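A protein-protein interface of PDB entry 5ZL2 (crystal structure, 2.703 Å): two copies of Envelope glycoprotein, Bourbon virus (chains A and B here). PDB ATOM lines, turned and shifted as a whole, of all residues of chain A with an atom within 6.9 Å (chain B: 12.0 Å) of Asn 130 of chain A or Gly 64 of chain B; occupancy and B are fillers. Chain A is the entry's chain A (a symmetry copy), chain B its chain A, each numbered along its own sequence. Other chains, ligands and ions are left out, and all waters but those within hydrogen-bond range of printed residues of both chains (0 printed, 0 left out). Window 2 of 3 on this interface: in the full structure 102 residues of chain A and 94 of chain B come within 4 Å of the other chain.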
ATOM      1  N   CYS A  56      14.586   0.782   1.955  1.00  0.00           N
ATOM      2  CA  CYS A  56      14.870  -0.134   3.049  1.00  0.00           C
ATOM      3  C   CYS A  56      15.893  -1.184   2.629  1.00  0.00           C
ATOM      4  O   CYS A  56      16.023  -1.509   1.447  1.00  0.00           O
ATOM      5  CB  CYS A  56      13.587  -0.832   3.519  1.00  0.00           C
ATOM      6  SG  CYS A  56      12.218   0.282   3.929  1.00  0.00           S
ATOM      7  N   ASN A  58      17.264  -5.105   4.170  1.00  0.00           N
ATOM      8  CA  ASN A  58      17.086  -6.206   5.115  1.00  0.00           C
ATOM      9  C   ASN A  58      18.299  -7.118   4.985  1.00  0.00           C
ATOM     10  O   ASN A  58      18.301  -8.055   4.184  1.00  0.00           O
ATOM     11  CB  ASN A  58      15.786  -6.957   4.844  1.00  0.00           C
ATOM     12  CG  ASN A  58      15.588  -8.147   5.765  1.00  0.00           C
ATOM     13  OD1 ASN A  58      16.409  -8.423   6.637  1.00  0.00           O
ATOM     14  ND2 ASN A  58      14.482  -8.855   5.576  1.00  0.00           N
ATOM     15  N   ASP A  99       7.206  -2.257  -3.984  1.00  0.00           N
ATOM     16  CA  ASP A  99       8.003  -3.467  -3.766  1.00  0.00           C
ATOM     17  C   ASP A  99       8.957  -3.725  -4.926  1.00  0.00           C
ATOM     18  O   ASP A  99       8.961  -4.790  -5.547  1.00  0.00           O
ATOM     19  CB  ASP A  99       7.115  -4.685  -3.514  1.00  0.00           C
ATOM     20  CG  ASP A  99       7.876  -5.838  -2.869  1.00  0.00           C
ATOM     21  OD1 ASP A  99       9.115  -5.742  -2.745  1.00  0.00           O
ATOM     22  OD2 ASP A  99       7.240  -6.842  -2.494  1.00  0.00           O
ATOM     23  N   SER A 127       5.509   0.765   3.108  1.00  0.00           N
ATOM     24  CA  SER A 127       6.913   0.400   3.236  1.00  0.00           C
ATOM     25  C   SER A 127       7.034  -1.117   3.295  1.00  0.00           C
ATOM     26  O   SER A 127       6.063  -1.829   3.551  1.00  0.00           O
ATOM     27  CB  SER A 127       7.558   1.032   4.475  1.00  0.00           C
ATOM     28  OG  SER A 127       8.879   0.558   4.647  1.00  0.00           O
ATOM     29  N   ASN A 128       8.255  -1.598   3.067  1.00  0.00           N
ATOM     30  CA  ASN A 128       8.508  -3.027   2.911  1.00  0.00           C
ATOM     31  C   ASN A 128       9.998  -3.292   3.079  1.00  0.00           C
ATOM     32  O   ASN A 128      10.818  -2.655   2.410  1.00  0.00           O
ATOM     33  CB  ASN A 128       8.032  -3.507   1.539  1.00  0.00           C
ATOM     34  CG  ASN A 128       7.731  -4.984   1.513  1.00  0.00           C
ATOM     35  OD1 ASN A 128       7.235  -5.545   2.491  1.00  0.00           O
ATOM     36  ND2 ASN A 128       8.025  -5.629   0.390  1.00  0.00           N
ATOM     37  N   ASN A 129      10.347  -4.216   3.973  1.00  0.00           N
ATOM     38  CA  ASN A 129      11.739  -4.604   4.193  1.00  0.00           C
ATOM     39  C   ASN A 129      11.856  -6.111   4.382  1.00  0.00           C
ATOM     40  O   ASN A 129      12.578  -6.592   5.263  1.00  0.00           O
ATOM     41  CB  ASN A 129      12.330  -3.864   5.390  1.00  0.00           C
ATOM     42  CG  ASN A 129      13.836  -3.896   5.404  1.00  0.00           C
ATOM     43  OD1 ASN A 129      14.472  -3.919   4.357  1.00  0.00           O
ATOM     44  ND2 ASN A 129      14.418  -3.907   6.594  1.00  0.00           N
ATOM     45  N   ASN A 130      11.151  -6.884   3.558  1.00  0.00           N
ATOM     46  CA  ASN A 130      11.056  -8.328   3.730  1.00  0.00           C
ATOM     47  C   ASN A 130      11.859  -9.097   2.683  1.00  0.00           C
ATOM     48  O   ASN A 130      11.535 -10.244   2.369  1.00  0.00           O
ATOM     49  CB  ASN A 130       9.596  -8.770   3.699  1.00  0.00           C
ATOM     50  CG  ASN A 130       8.942  -8.502   2.364  1.00  0.00           C
ATOM     51  OD1 ASN A 130       9.233  -7.501   1.711  1.00  0.00           O
ATOM     52  ND2 ASN A 130       8.062  -9.402   1.943  1.00  0.00           N
ATOM     53  N   HIS A 131      12.907  -8.486   2.136  1.00  0.00           N
ATOM     54  CA  HIS A 131      13.780  -9.140   1.166  1.00  0.00           C
ATOM     55  C   HIS A 131      15.184  -9.190   1.751  1.00  0.00           C
ATOM     56  O   HIS A 131      15.850  -8.155   1.873  1.00  0.00           O
ATOM     57  CB  HIS A 131      13.763  -8.405  -0.174  1.00  0.00           C
ATOM     58  CG  HIS A 131      12.467  -8.524  -0.910  1.00  0.00           C
ATOM     59  ND1 HIS A 131      11.935  -9.739  -1.286  1.00  0.00           N
ATOM     60  CD2 HIS A 131      11.596  -7.582  -1.343  1.00  0.00           C
ATOM     61  CE1 HIS A 131      10.793  -9.538  -1.918  1.00  0.00           C
ATOM     62  NE2 HIS A 131      10.565  -8.239  -1.966  1.00  0.00           N
ATOM     63  N   PHE A 132      15.640 -10.390   2.100  1.00  0.00           N
ATOM     64  CA  PHE A 132      16.890 -10.512   2.834  1.00  0.00           C
ATOM     65  C   PHE A 132      18.091 -10.211   1.947  1.00  0.00           C
ATOM     66  O   PHE A 132      18.119 -10.565   0.764  1.00  0.00           O
ATOM     67  CB  PHE A 132      17.035 -11.903   3.443  1.00  0.00           C
ATOM     68  CG  PHE A 132      18.206 -12.022   4.371  1.00  0.00           C
ATOM     69  CD1 PHE A 132      18.119 -11.570   5.678  1.00  0.00           C
ATOM     70  CD2 PHE A 132      19.407 -12.554   3.930  1.00  0.00           C
ATOM     71  CE1 PHE A 132      19.200 -11.665   6.531  1.00  0.00           C
ATOM     72  CE2 PHE A 132      20.494 -12.652   4.778  1.00  0.00           C
ATOM     73  CZ  PHE A 132      20.390 -12.207   6.079  1.00  0.00           C
ATOM     74  N   HIS A 134      18.944  -7.573   0.658  1.00  0.00           N
ATOM     75  CA  HIS A 134      18.482  -6.855  -0.516  1.00  0.00           C
ATOM     76  C   HIS A 134      17.829  -5.551  -0.087  1.00  0.00           C
ATOM     77  O   HIS A 134      17.338  -5.417   1.036  1.00  0.00           O
ATOM     78  CB  HIS A 134      17.496  -7.701  -1.331  1.00  0.00           C
ATOM     79  CG  HIS A 134      18.153  -8.755  -2.163  1.00  0.00           C
ATOM     80  ND1 HIS A 134      19.521  -8.902  -2.234  1.00  0.00           N
ATOM     81  CD2 HIS A 134      17.630  -9.705  -2.973  1.00  0.00           C
ATOM     82  CE1 HIS A 134      19.813  -9.900  -3.049  1.00  0.00           C
ATOM     83  NE2 HIS A 134      18.684 -10.402  -3.513  1.00  0.00           N
ATOM     84  N   THR A 136      14.827  -2.586  -0.782  1.00  0.00           N
ATOM     85  CA  THR A 136      13.444  -2.501  -1.235  1.00  0.00           C
ATOM     86  C   THR A 136      13.056  -1.033  -1.307  1.00  0.00           C
ATOM     87  O   THR A 136      13.356  -0.265  -0.390  1.00  0.00           O
ATOM     88  CB  THR A 136      12.487  -3.260  -0.306  1.00  0.00           C
ATOM     89  OG1 THR A 136      12.890  -4.631  -0.213  1.00  0.00           O
ATOM     90  CG2 THR A 136      11.063  -3.200  -0.840  1.00  0.00           C
ATOM     91  N   ASN A 443       1.703  -2.155   4.261  1.00  0.00           N
ATOM     92  CA  ASN A 443       2.733  -3.122   3.906  1.00  0.00           C
ATOM     93  C   ASN A 443       2.640  -3.405   2.411  1.00  0.00           C
ATOM     94  O   ASN A 443       1.675  -4.019   1.947  1.00  0.00           O
ATOM     95  CB  ASN A 443       2.596  -4.404   4.722  1.00  0.00           C
ATOM     96  CG  ASN A 443       3.905  -5.155   4.850  1.00  0.00           C
ATOM     97  OD1 ASN A 443       4.601  -5.392   3.860  1.00  0.00           O
ATOM     98  ND2 ASN A 443       4.250  -5.535   6.077  1.00  0.00           N
ATOM     99  N   GLY A 444       3.645  -2.959   1.666  1.00  0.00           N
ATOM    100  CA  GLY A 444       3.688  -3.188   0.238  1.00  0.00           C
ATOM    101  C   GLY A 444       4.232  -4.553  -0.122  1.00  0.00           C
ATOM    102  O   GLY A 444       4.829  -4.729  -1.188  1.00  0.00           O
ATOM    103  N   GLY A 445       4.039  -5.527   0.762  1.00  0.00           N
ATOM    104  CA  GLY A 445       4.450  -6.893   0.499  1.00  0.00           C
ATOM    105  C   GLY A 445       3.611  -7.570  -0.571  1.00  0.00           C
ATOM    106  O   GLY A 445       2.425  -7.835  -0.374  1.00  0.00           O
ATOM    107  N   TYR B  55      -1.838  -7.158  12.331  1.00  0.00           N
ATOM    108  CA  TYR B  55      -1.595  -8.596  12.274  1.00  0.00           C
ATOM    109  C   TYR B  55      -0.157  -8.829  11.815  1.00  0.00           C
ATOM    110  O   TYR B  55       0.161  -8.664  10.633  1.00  0.00           O
ATOM    111  CB  TYR B  55      -2.595  -9.269  11.337  1.00  0.00           C
ATOM    112  CG  TYR B  55      -2.533 -10.773  11.352  1.00  0.00           C
ATOM    113  CD1 TYR B  55      -2.936 -11.489  12.470  1.00  0.00           C
ATOM    114  CD2 TYR B  55      -2.079 -11.480  10.247  1.00  0.00           C
ATOM    115  CE1 TYR B  55      -2.883 -12.868  12.494  1.00  0.00           C
ATOM    116  CE2 TYR B  55      -2.023 -12.859  10.259  1.00  0.00           C
ATOM    117  CZ  TYR B  55      -2.427 -13.548  11.387  1.00  0.00           C
ATOM    118  OH  TYR B  55      -2.375 -14.924  11.405  1.00  0.00           O
ATOM    119  N   CYS B  56       0.707  -9.213  12.751  1.00  0.00           N
ATOM    120  CA  CYS B  56       2.138  -9.316  12.511  1.00  0.00           C
ATOM    121  C   CYS B  56       2.604 -10.764  12.599  1.00  0.00           C
ATOM    122  O   CYS B  56       1.989 -11.590  13.278  1.00  0.00           O
ATOM    123  CB  CYS B  56       2.920  -8.466  13.521  1.00  0.00           C
ATOM    124  SG  CYS B  56       2.392  -6.736  13.636  1.00  0.00           S
ATOM    125  N   TYR B  57       3.707 -11.061  11.910  1.00  0.00           N
ATOM    126  CA  TYR B  57       4.355 -12.365  11.995  1.00  0.00           C
ATOM    127  C   TYR B  57       5.862 -12.175  12.076  1.00  0.00           C
ATOM    128  O   TYR B  57       6.442 -11.424  11.286  1.00  0.00           O
ATOM    129  CB  TYR B  57       4.005 -13.255  10.798  1.00  0.00           C
ATOM    130  CG  TYR B  57       4.678 -14.612  10.834  1.00  0.00           C
ATOM    131  CD1 TYR B  57       4.241 -15.608  11.698  1.00  0.00           C
ATOM    132  CD2 TYR B  57       5.752 -14.896   9.999  1.00  0.00           C
ATOM    133  CE1 TYR B  57       4.856 -16.847  11.729  1.00  0.00           C
ATOM    134  CE2 TYR B  57       6.371 -16.130  10.022  1.00  0.00           C
ATOM    135  CZ  TYR B  57       5.920 -17.100  10.887  1.00  0.00           C
ATOM    136  OH  TYR B  57       6.545 -18.325  10.901  1.00  0.00           O
ATOM    137  N   ASN B  58       6.487 -12.853  13.035  1.00  0.00           N
ATOM    138  CA  ASN B  58       7.925 -12.774  13.280  1.00  0.00           C
ATOM    139  C   ASN B  58       8.508 -14.157  13.020  1.00  0.00           C
ATOM    140  O   ASN B  58       8.589 -14.987  13.929  1.00  0.00           O
ATOM    141  CB  ASN B  58       8.214 -12.298  14.701  1.00  0.00           C
ATOM    142  CG  ASN B  58       9.697 -12.259  15.021  1.00  0.00           C
ATOM    143  OD1 ASN B  58      10.540 -12.566  14.181  1.00  0.00           O
ATOM    144  ND2 ASN B  58      10.020 -11.866  16.246  1.00  0.00           N
ATOM    145  N   GLY B  59       8.918 -14.396  11.779  1.00  0.00           N
ATOM    146  CA  GLY B  59       9.561 -15.643  11.424  1.00  0.00           C
ATOM    147  C   GLY B  59      10.999 -15.435  11.002  1.00  0.00           C
ATOM    148  O   GLY B  59      11.513 -16.156  10.144  1.00  0.00           O
ATOM    149  N   GLY B  60      11.656 -14.449  11.597  1.00  0.00           N
ATOM    150  CA  GLY B  60      13.034 -14.153  11.280  1.00  0.00           C
ATOM    151  C   GLY B  60      13.180 -13.332  10.011  1.00  0.00           C
ATOM    152  O   GLY B  60      12.302 -13.288   9.151  1.00  0.00           O
ATOM    153  N   SER B  61      14.334 -12.672   9.899  1.00  0.00           N
ATOM    154  CA  SER B  61      14.588 -11.792   8.766  1.00  0.00           C
ATOM    155  C   SER B  61      14.697 -12.547   7.449  1.00  0.00           C
ATOM    156  O   SER B  61      14.546 -11.937   6.386  1.00  0.00           O
ATOM    157  CB  SER B  61      15.863 -10.982   9.005  1.00  0.00           C
ATOM    158  OG  SER B  61      15.770 -10.230  10.203  1.00  0.00           O
ATOM    159  N   LEU B  62      14.951 -13.856   7.491  1.00  0.00           N
ATOM    160  CA  LEU B  62      15.012 -14.625   6.254  1.00  0.00           C
ATOM    161  C   LEU B  62      13.626 -14.863   5.670  1.00  0.00           C
ATOM    162  O   LEU B  62      13.477 -14.930   4.445  1.00  0.00           O
ATOM    163  CB  LEU B  62      15.720 -15.960   6.491  1.00  0.00           C
ATOM    164  CG  LEU B  62      17.234 -15.919   6.733  1.00  0.00           C
ATOM    165  CD1 LEU B  62      17.778 -17.315   6.998  1.00  0.00           C
ATOM    166  CD2 LEU B  62      17.957 -15.283   5.560  1.00  0.00           C
ATOM    167  N   ASP B  63      12.607 -14.990   6.516  1.00  0.00           N
ATOM    168  CA  ASP B  63      11.275 -15.322   6.029  1.00  0.00           C
ATOM    169  C   ASP B  63      10.625 -14.115   5.365  1.00  0.00           C
ATOM    170  O   ASP B  63      10.540 -13.034   5.956  1.00  0.00           O
ATOM    171  CB  ASP B  63      10.398 -15.827   7.173  1.00  0.00           C
ATOM    172  CG  ASP B  63       9.062 -16.350   6.692  1.00  0.00           C
ATOM    173  OD1 ASP B  63       8.924 -16.615   5.480  1.00  0.00           O
ATOM    174  OD2 ASP B  63       8.144 -16.491   7.523  1.00  0.00           O
ATOM    175  N   GLY B  64      10.151 -14.311   4.133  1.00  0.00           N
ATOM    176  CA  GLY B  64       9.521 -13.233   3.394  1.00  0.00           C
ATOM    177  C   GLY B  64       8.239 -12.726   4.019  1.00  0.00           C
ATOM    178  O   GLY B  64       7.808 -11.610   3.707  1.00  0.00           O
ATOM    179  N   ASN B  65       7.623 -13.512   4.898  1.00  0.00           N
ATOM    180  CA  ASN B  65       6.374 -13.140   5.543  1.00  0.00           C
ATOM    181  C   ASN B  65       6.580 -12.399   6.860  1.00  0.00           C
ATOM    182  O   ASN B  65       5.610 -12.175   7.590  1.00  0.00           O
ATOM    183  CB  ASN B  65       5.521 -14.386   5.780  1.00  0.00           C
ATOM    184  CG  ASN B  65       5.268 -15.162   4.508  1.00  0.00           C
ATOM    185  OD1 ASN B  65       5.165 -14.582   3.428  1.00  0.00           O
ATOM    186  ND2 ASN B  65       5.172 -16.482   4.626  1.00  0.00           N
ATOM    187  N   THR B  66       7.815 -12.016   7.176  1.00  0.00           N
ATOM    188  CA  THR B  66       8.118 -11.350   8.437  1.00  0.00           C
ATOM    189  C   THR B  66       7.797  -9.863   8.328  1.00  0.00           C
ATOM    190  O   THR B  66       8.357  -9.155   7.484  1.00  0.00           O
ATOM    191  CB  THR B  66       9.583 -11.571   8.805  1.00  0.00           C
ATOM    192  OG1 THR B  66       9.761 -12.917   9.266  1.00  0.00           O
ATOM    193  CG2 THR B  66      10.019 -10.608   9.897  1.00  0.00           C
ATOM    194  N   GLY B  67       6.905  -9.394   9.182  1.00  0.00           N
ATOM    195  CA  GLY B  67       6.433  -8.027   9.129  1.00  0.00           C
ATOM    196  C   GLY B  67       5.003  -7.963   9.626  1.00  0.00           C
ATOM    197  O   GLY B  67       4.442  -8.953  10.092  1.00  0.00           O
ATOM    198  N   CYS B  68       4.421  -6.771   9.517  1.00  0.00           N
ATOM    199  CA  CYS B  68       3.066  -6.524   9.985  1.00  0.00           C
ATOM    200  C   CYS B  68       2.152  -6.196   8.813  1.00  0.00           C
ATOM    201  O   CYS B  68       2.599  -5.706   7.770  1.00  0.00           O
ATOM    202  CB  CYS B  68       3.017  -5.376  10.999  1.00  0.00           C
ATOM    203  SG  CYS B  68       3.800  -5.731  12.577  1.00  0.00           S
ATOM    204  N   TYR B  69       0.866  -6.485   9.000  1.00  0.00           N
ATOM    205  CA  TYR B  69      -0.201  -6.053   8.103  1.00  0.00           C
ATOM    206  C   TYR B  69      -1.168  -5.211   8.928  1.00  0.00           C
ATOM    207  O   TYR B  69      -1.941  -5.750   9.728  1.00  0.00           O
ATOM    208  CB  TYR B  69      -0.912  -7.247   7.465  1.00  0.00           C
ATOM    209  CG  TYR B  69      -0.302  -7.731   6.165  1.00  0.00           C
ATOM    210  CD1 TYR B  69       0.937  -7.273   5.739  1.00  0.00           C
ATOM    211  CD2 TYR B  69      -0.967  -8.650   5.362  1.00  0.00           C
ATOM    212  CE1 TYR B  69       1.497  -7.715   4.549  1.00  0.00           C
ATOM    213  CE2 TYR B  69      -0.417  -9.098   4.171  1.00  0.00           C
ATOM    214  CZ  TYR B  69       0.815  -8.625   3.772  1.00  0.00           C
ATOM    215  OH  TYR B  69       1.367  -9.063   2.591  1.00  0.00           O
ATOM    216  N   ASN B 129       5.502  -7.436  17.320  1.00  0.00           N
ATOM    217  CA  ASN B 129       5.975  -8.536  16.481  1.00  0.00           C
ATOM    218  C   ASN B 129       7.166  -9.234  17.126  1.00  0.00           C
ATOM    219  O   ASN B 129       8.155  -9.560  16.460  1.00  0.00           O
ATOM    220  CB  ASN B 129       6.334  -8.041  15.081  1.00  0.00           C
ATOM    221  CG  ASN B 129       6.415  -9.159  14.076  1.00  0.00           C
ATOM    222  OD1 ASN B 129       5.702 -10.151  14.181  1.00  0.00           O
ATOM    223  ND2 ASN B 129       7.293  -9.011  13.095  1.00  0.00           N
ATOM    224  N   PHE B 132       8.641 -15.136  18.034  1.00  0.00           N
ATOM    225  CA  PHE B 132       9.292 -15.755  16.890  1.00  0.00           C
ATOM    226  C   PHE B 132       8.487 -16.933  16.358  1.00  0.00           C
ATOM    227  O   PHE B 132       7.888 -17.697  17.122  1.00  0.00           O
ATOM    228  CB  PHE B 132      10.704 -16.213  17.244  1.00  0.00           C
ATOM    229  CG  PHE B 132      11.489 -16.678  16.054  1.00  0.00           C
ATOM    230  CD1 PHE B 132      12.106 -15.764  15.215  1.00  0.00           C
ATOM    231  CD2 PHE B 132      11.583 -18.028  15.752  1.00  0.00           C
ATOM    232  CE1 PHE B 132      12.817 -16.188  14.110  1.00  0.00           C
ATOM    233  CE2 PHE B 132      12.293 -18.460  14.649  1.00  0.00           C
ATOM    234  CZ  PHE B 132      12.910 -17.539  13.826  1.00  0.00           C
ATOM    235  N   ALA B 133       8.492 -17.076  15.028  1.00  0.00           N
ATOM    236  CA  ALA B 133       7.769 -18.134  14.321  1.00  0.00           C
ATOM    237  C   ALA B 133       6.287 -18.134  14.678  1.00  0.00           C
ATOM    238  O   ALA B 133       5.630 -19.177  14.662  1.00  0.00           O
ATOM    239  CB  ALA B 133       8.387 -19.509  14.591  1.00  0.00           C
ATOM    240  N   HIS B 134       5.751 -16.960  14.994  1.00  0.00           N
ATOM    241  CA  HIS B 134       4.395 -16.858  15.501  1.00  0.00           C
ATOM    242  C   HIS B 134       3.770 -15.559  15.020  1.00  0.00           C
ATOM    243  O   HIS B 134       4.465 -14.585  14.718  1.00  0.00           O
ATOM    244  CB  HIS B 134       4.371 -16.925  17.033  1.00  0.00           C
ATOM    245  CG  HIS B 134       4.531 -18.308  17.578  1.00  0.00           C
ATOM    246  ND1 HIS B 134       4.629 -19.419  16.769  1.00  0.00           N
ATOM    247  CD2 HIS B 134       4.598 -18.762  18.851  1.00  0.00           C
ATOM    248  CE1 HIS B 134       4.751 -20.499  17.520  1.00  0.00           C
ATOM    249  NE2 HIS B 134       4.733 -20.127  18.787  1.00  0.00           N
ATOM    250  N   HIS B 135       2.445 -15.556  14.953  1.00  0.00           N
ATOM    251  CA  HIS B 135       1.701 -14.348  14.643  1.00  0.00           C
ATOM    252  C   HIS B 135       1.356 -13.601  15.926  1.00  0.00           C
ATOM    253  O   HIS B 135       1.325 -14.173  17.016  1.00  0.00           O
ATOM    254  CB  HIS B 135       0.425 -14.679  13.872  1.00  0.00           C
ATOM    255  CG  HIS B 135       0.668 -15.153  12.473  1.00  0.00           C
ATOM    256  ND1 HIS B 135       0.746 -14.293  11.399  1.00  0.00           N
ATOM    257  CD2 HIS B 135       0.842 -16.399  11.972  1.00  0.00           C
ATOM    258  CE1 HIS B 135       0.963 -14.988  10.297  1.00  0.00           C
ATOM    259  NE2 HIS B 135       1.025 -16.268  10.617  1.00  0.00           N
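Hydrophobic or aromatic side chains of chain B that line the printed part of chain A: Leu 62 and Tyr 69. Printed residues of chain A that touch a printed residue of chain B: Asn 58, Asn 130, Phe 132, Asn 443 and Gly 445. Hydrophobic or aromatic side chains of chain A that line the printed part of chain B: Phe 132. Among the printed residues, 7 pairs touch across the chains. Among the printed residues, no Asp or Glu carboxylate lies within 4 Å of a Lys or Arg side-chain nitrogen of the other chain.
Positions printed for both chains: 56, 58, 129, 132 and 134.
Printed residues of chain B within 4 Å of Asn 58 of chain A: Ser 61. Of the printed residues of chain B, Asn 130 of chain A touches Gly 64 (2.8 Å). No residue of chain B comes within 4 Å of His 131 of chain A. Of the printed residues of chain B, Phe 132 of chain A touches Ser 61 (3.7 Å) and Leu 62 (3.5 Å). Of the printed residues of chain B, Asn 443 of chain A touches Cys 68 (2.4 Å) and Tyr 69 (3.5 Å). Gly 444 of chain A touches none of the printed residues of chain B. Gly 64 of chain B touches one residue of chain A. The nearest printed residue of chain B that does not touch Asn 130 of chain A is Thr 66 of chain B (4.001 Å). The nearest printed residue of chain B that does not touch Asn 443 of chain A is Gly 67 of chain B (4.4 Å).
The backbone carbonyl oxygen (O) of Ser 61 of chain B is in hydrogen-bond range of the side-chain amide nitrogen (ND2) of Asn 58 of chain A (3.2 Å). O of Gly 64 of chain B is in hydrogen-bond range of ND2 of Asn 130 of chain A, 2.8 Å away. OH of Tyr 69 of chain B sits at hydrogen-bond distance from O of Gly 445 of chain A, 3.4 Å away. ND2 of Asn 443 of chain A sits close to O of Cys 68 of chain B, at 2.4 Å.
The backbone carbonyl oxygen (O) of Tyr 55 of chain B sits at hydrogen-bond distance from the backbone NH (N) of Tyr 69 of chain B (2.8 Å). The side-chain sulfur of Cys 56 of chain B is disulfide-bonded to the side-chain sulfur of Cys 68 of chain B, 2.0 Å away. O of Asn 129 of chain A sits at hydrogen-bond distance from ND2 of Asn 58 of chain A, 3.0 Å away. N of Asn 58 of chain A is in hydrogen-bond range of O of His 134 of chain A, 3.2 Å away. The side-chain amide oxygen (OD1) of Asn 128 of chain A lies close to the side-chain amide oxygen (OD1) of Asn 443 of chain A (3.0 Å). The side-chain amide oxygen (OD1) of Asn 443 of chain A lies close to the backbone NH (N) of Gly 445 of chain A (3.2 Å).
O of Ser 61 of chain B touches CD1 of Phe 132 of chain A (3.7 Å). Phe 132 of chain A touches Leu 62 of chain B. Asn 443 of chain A touches Tyr 69 of chain B (CB to CD1, 3.5 Å).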
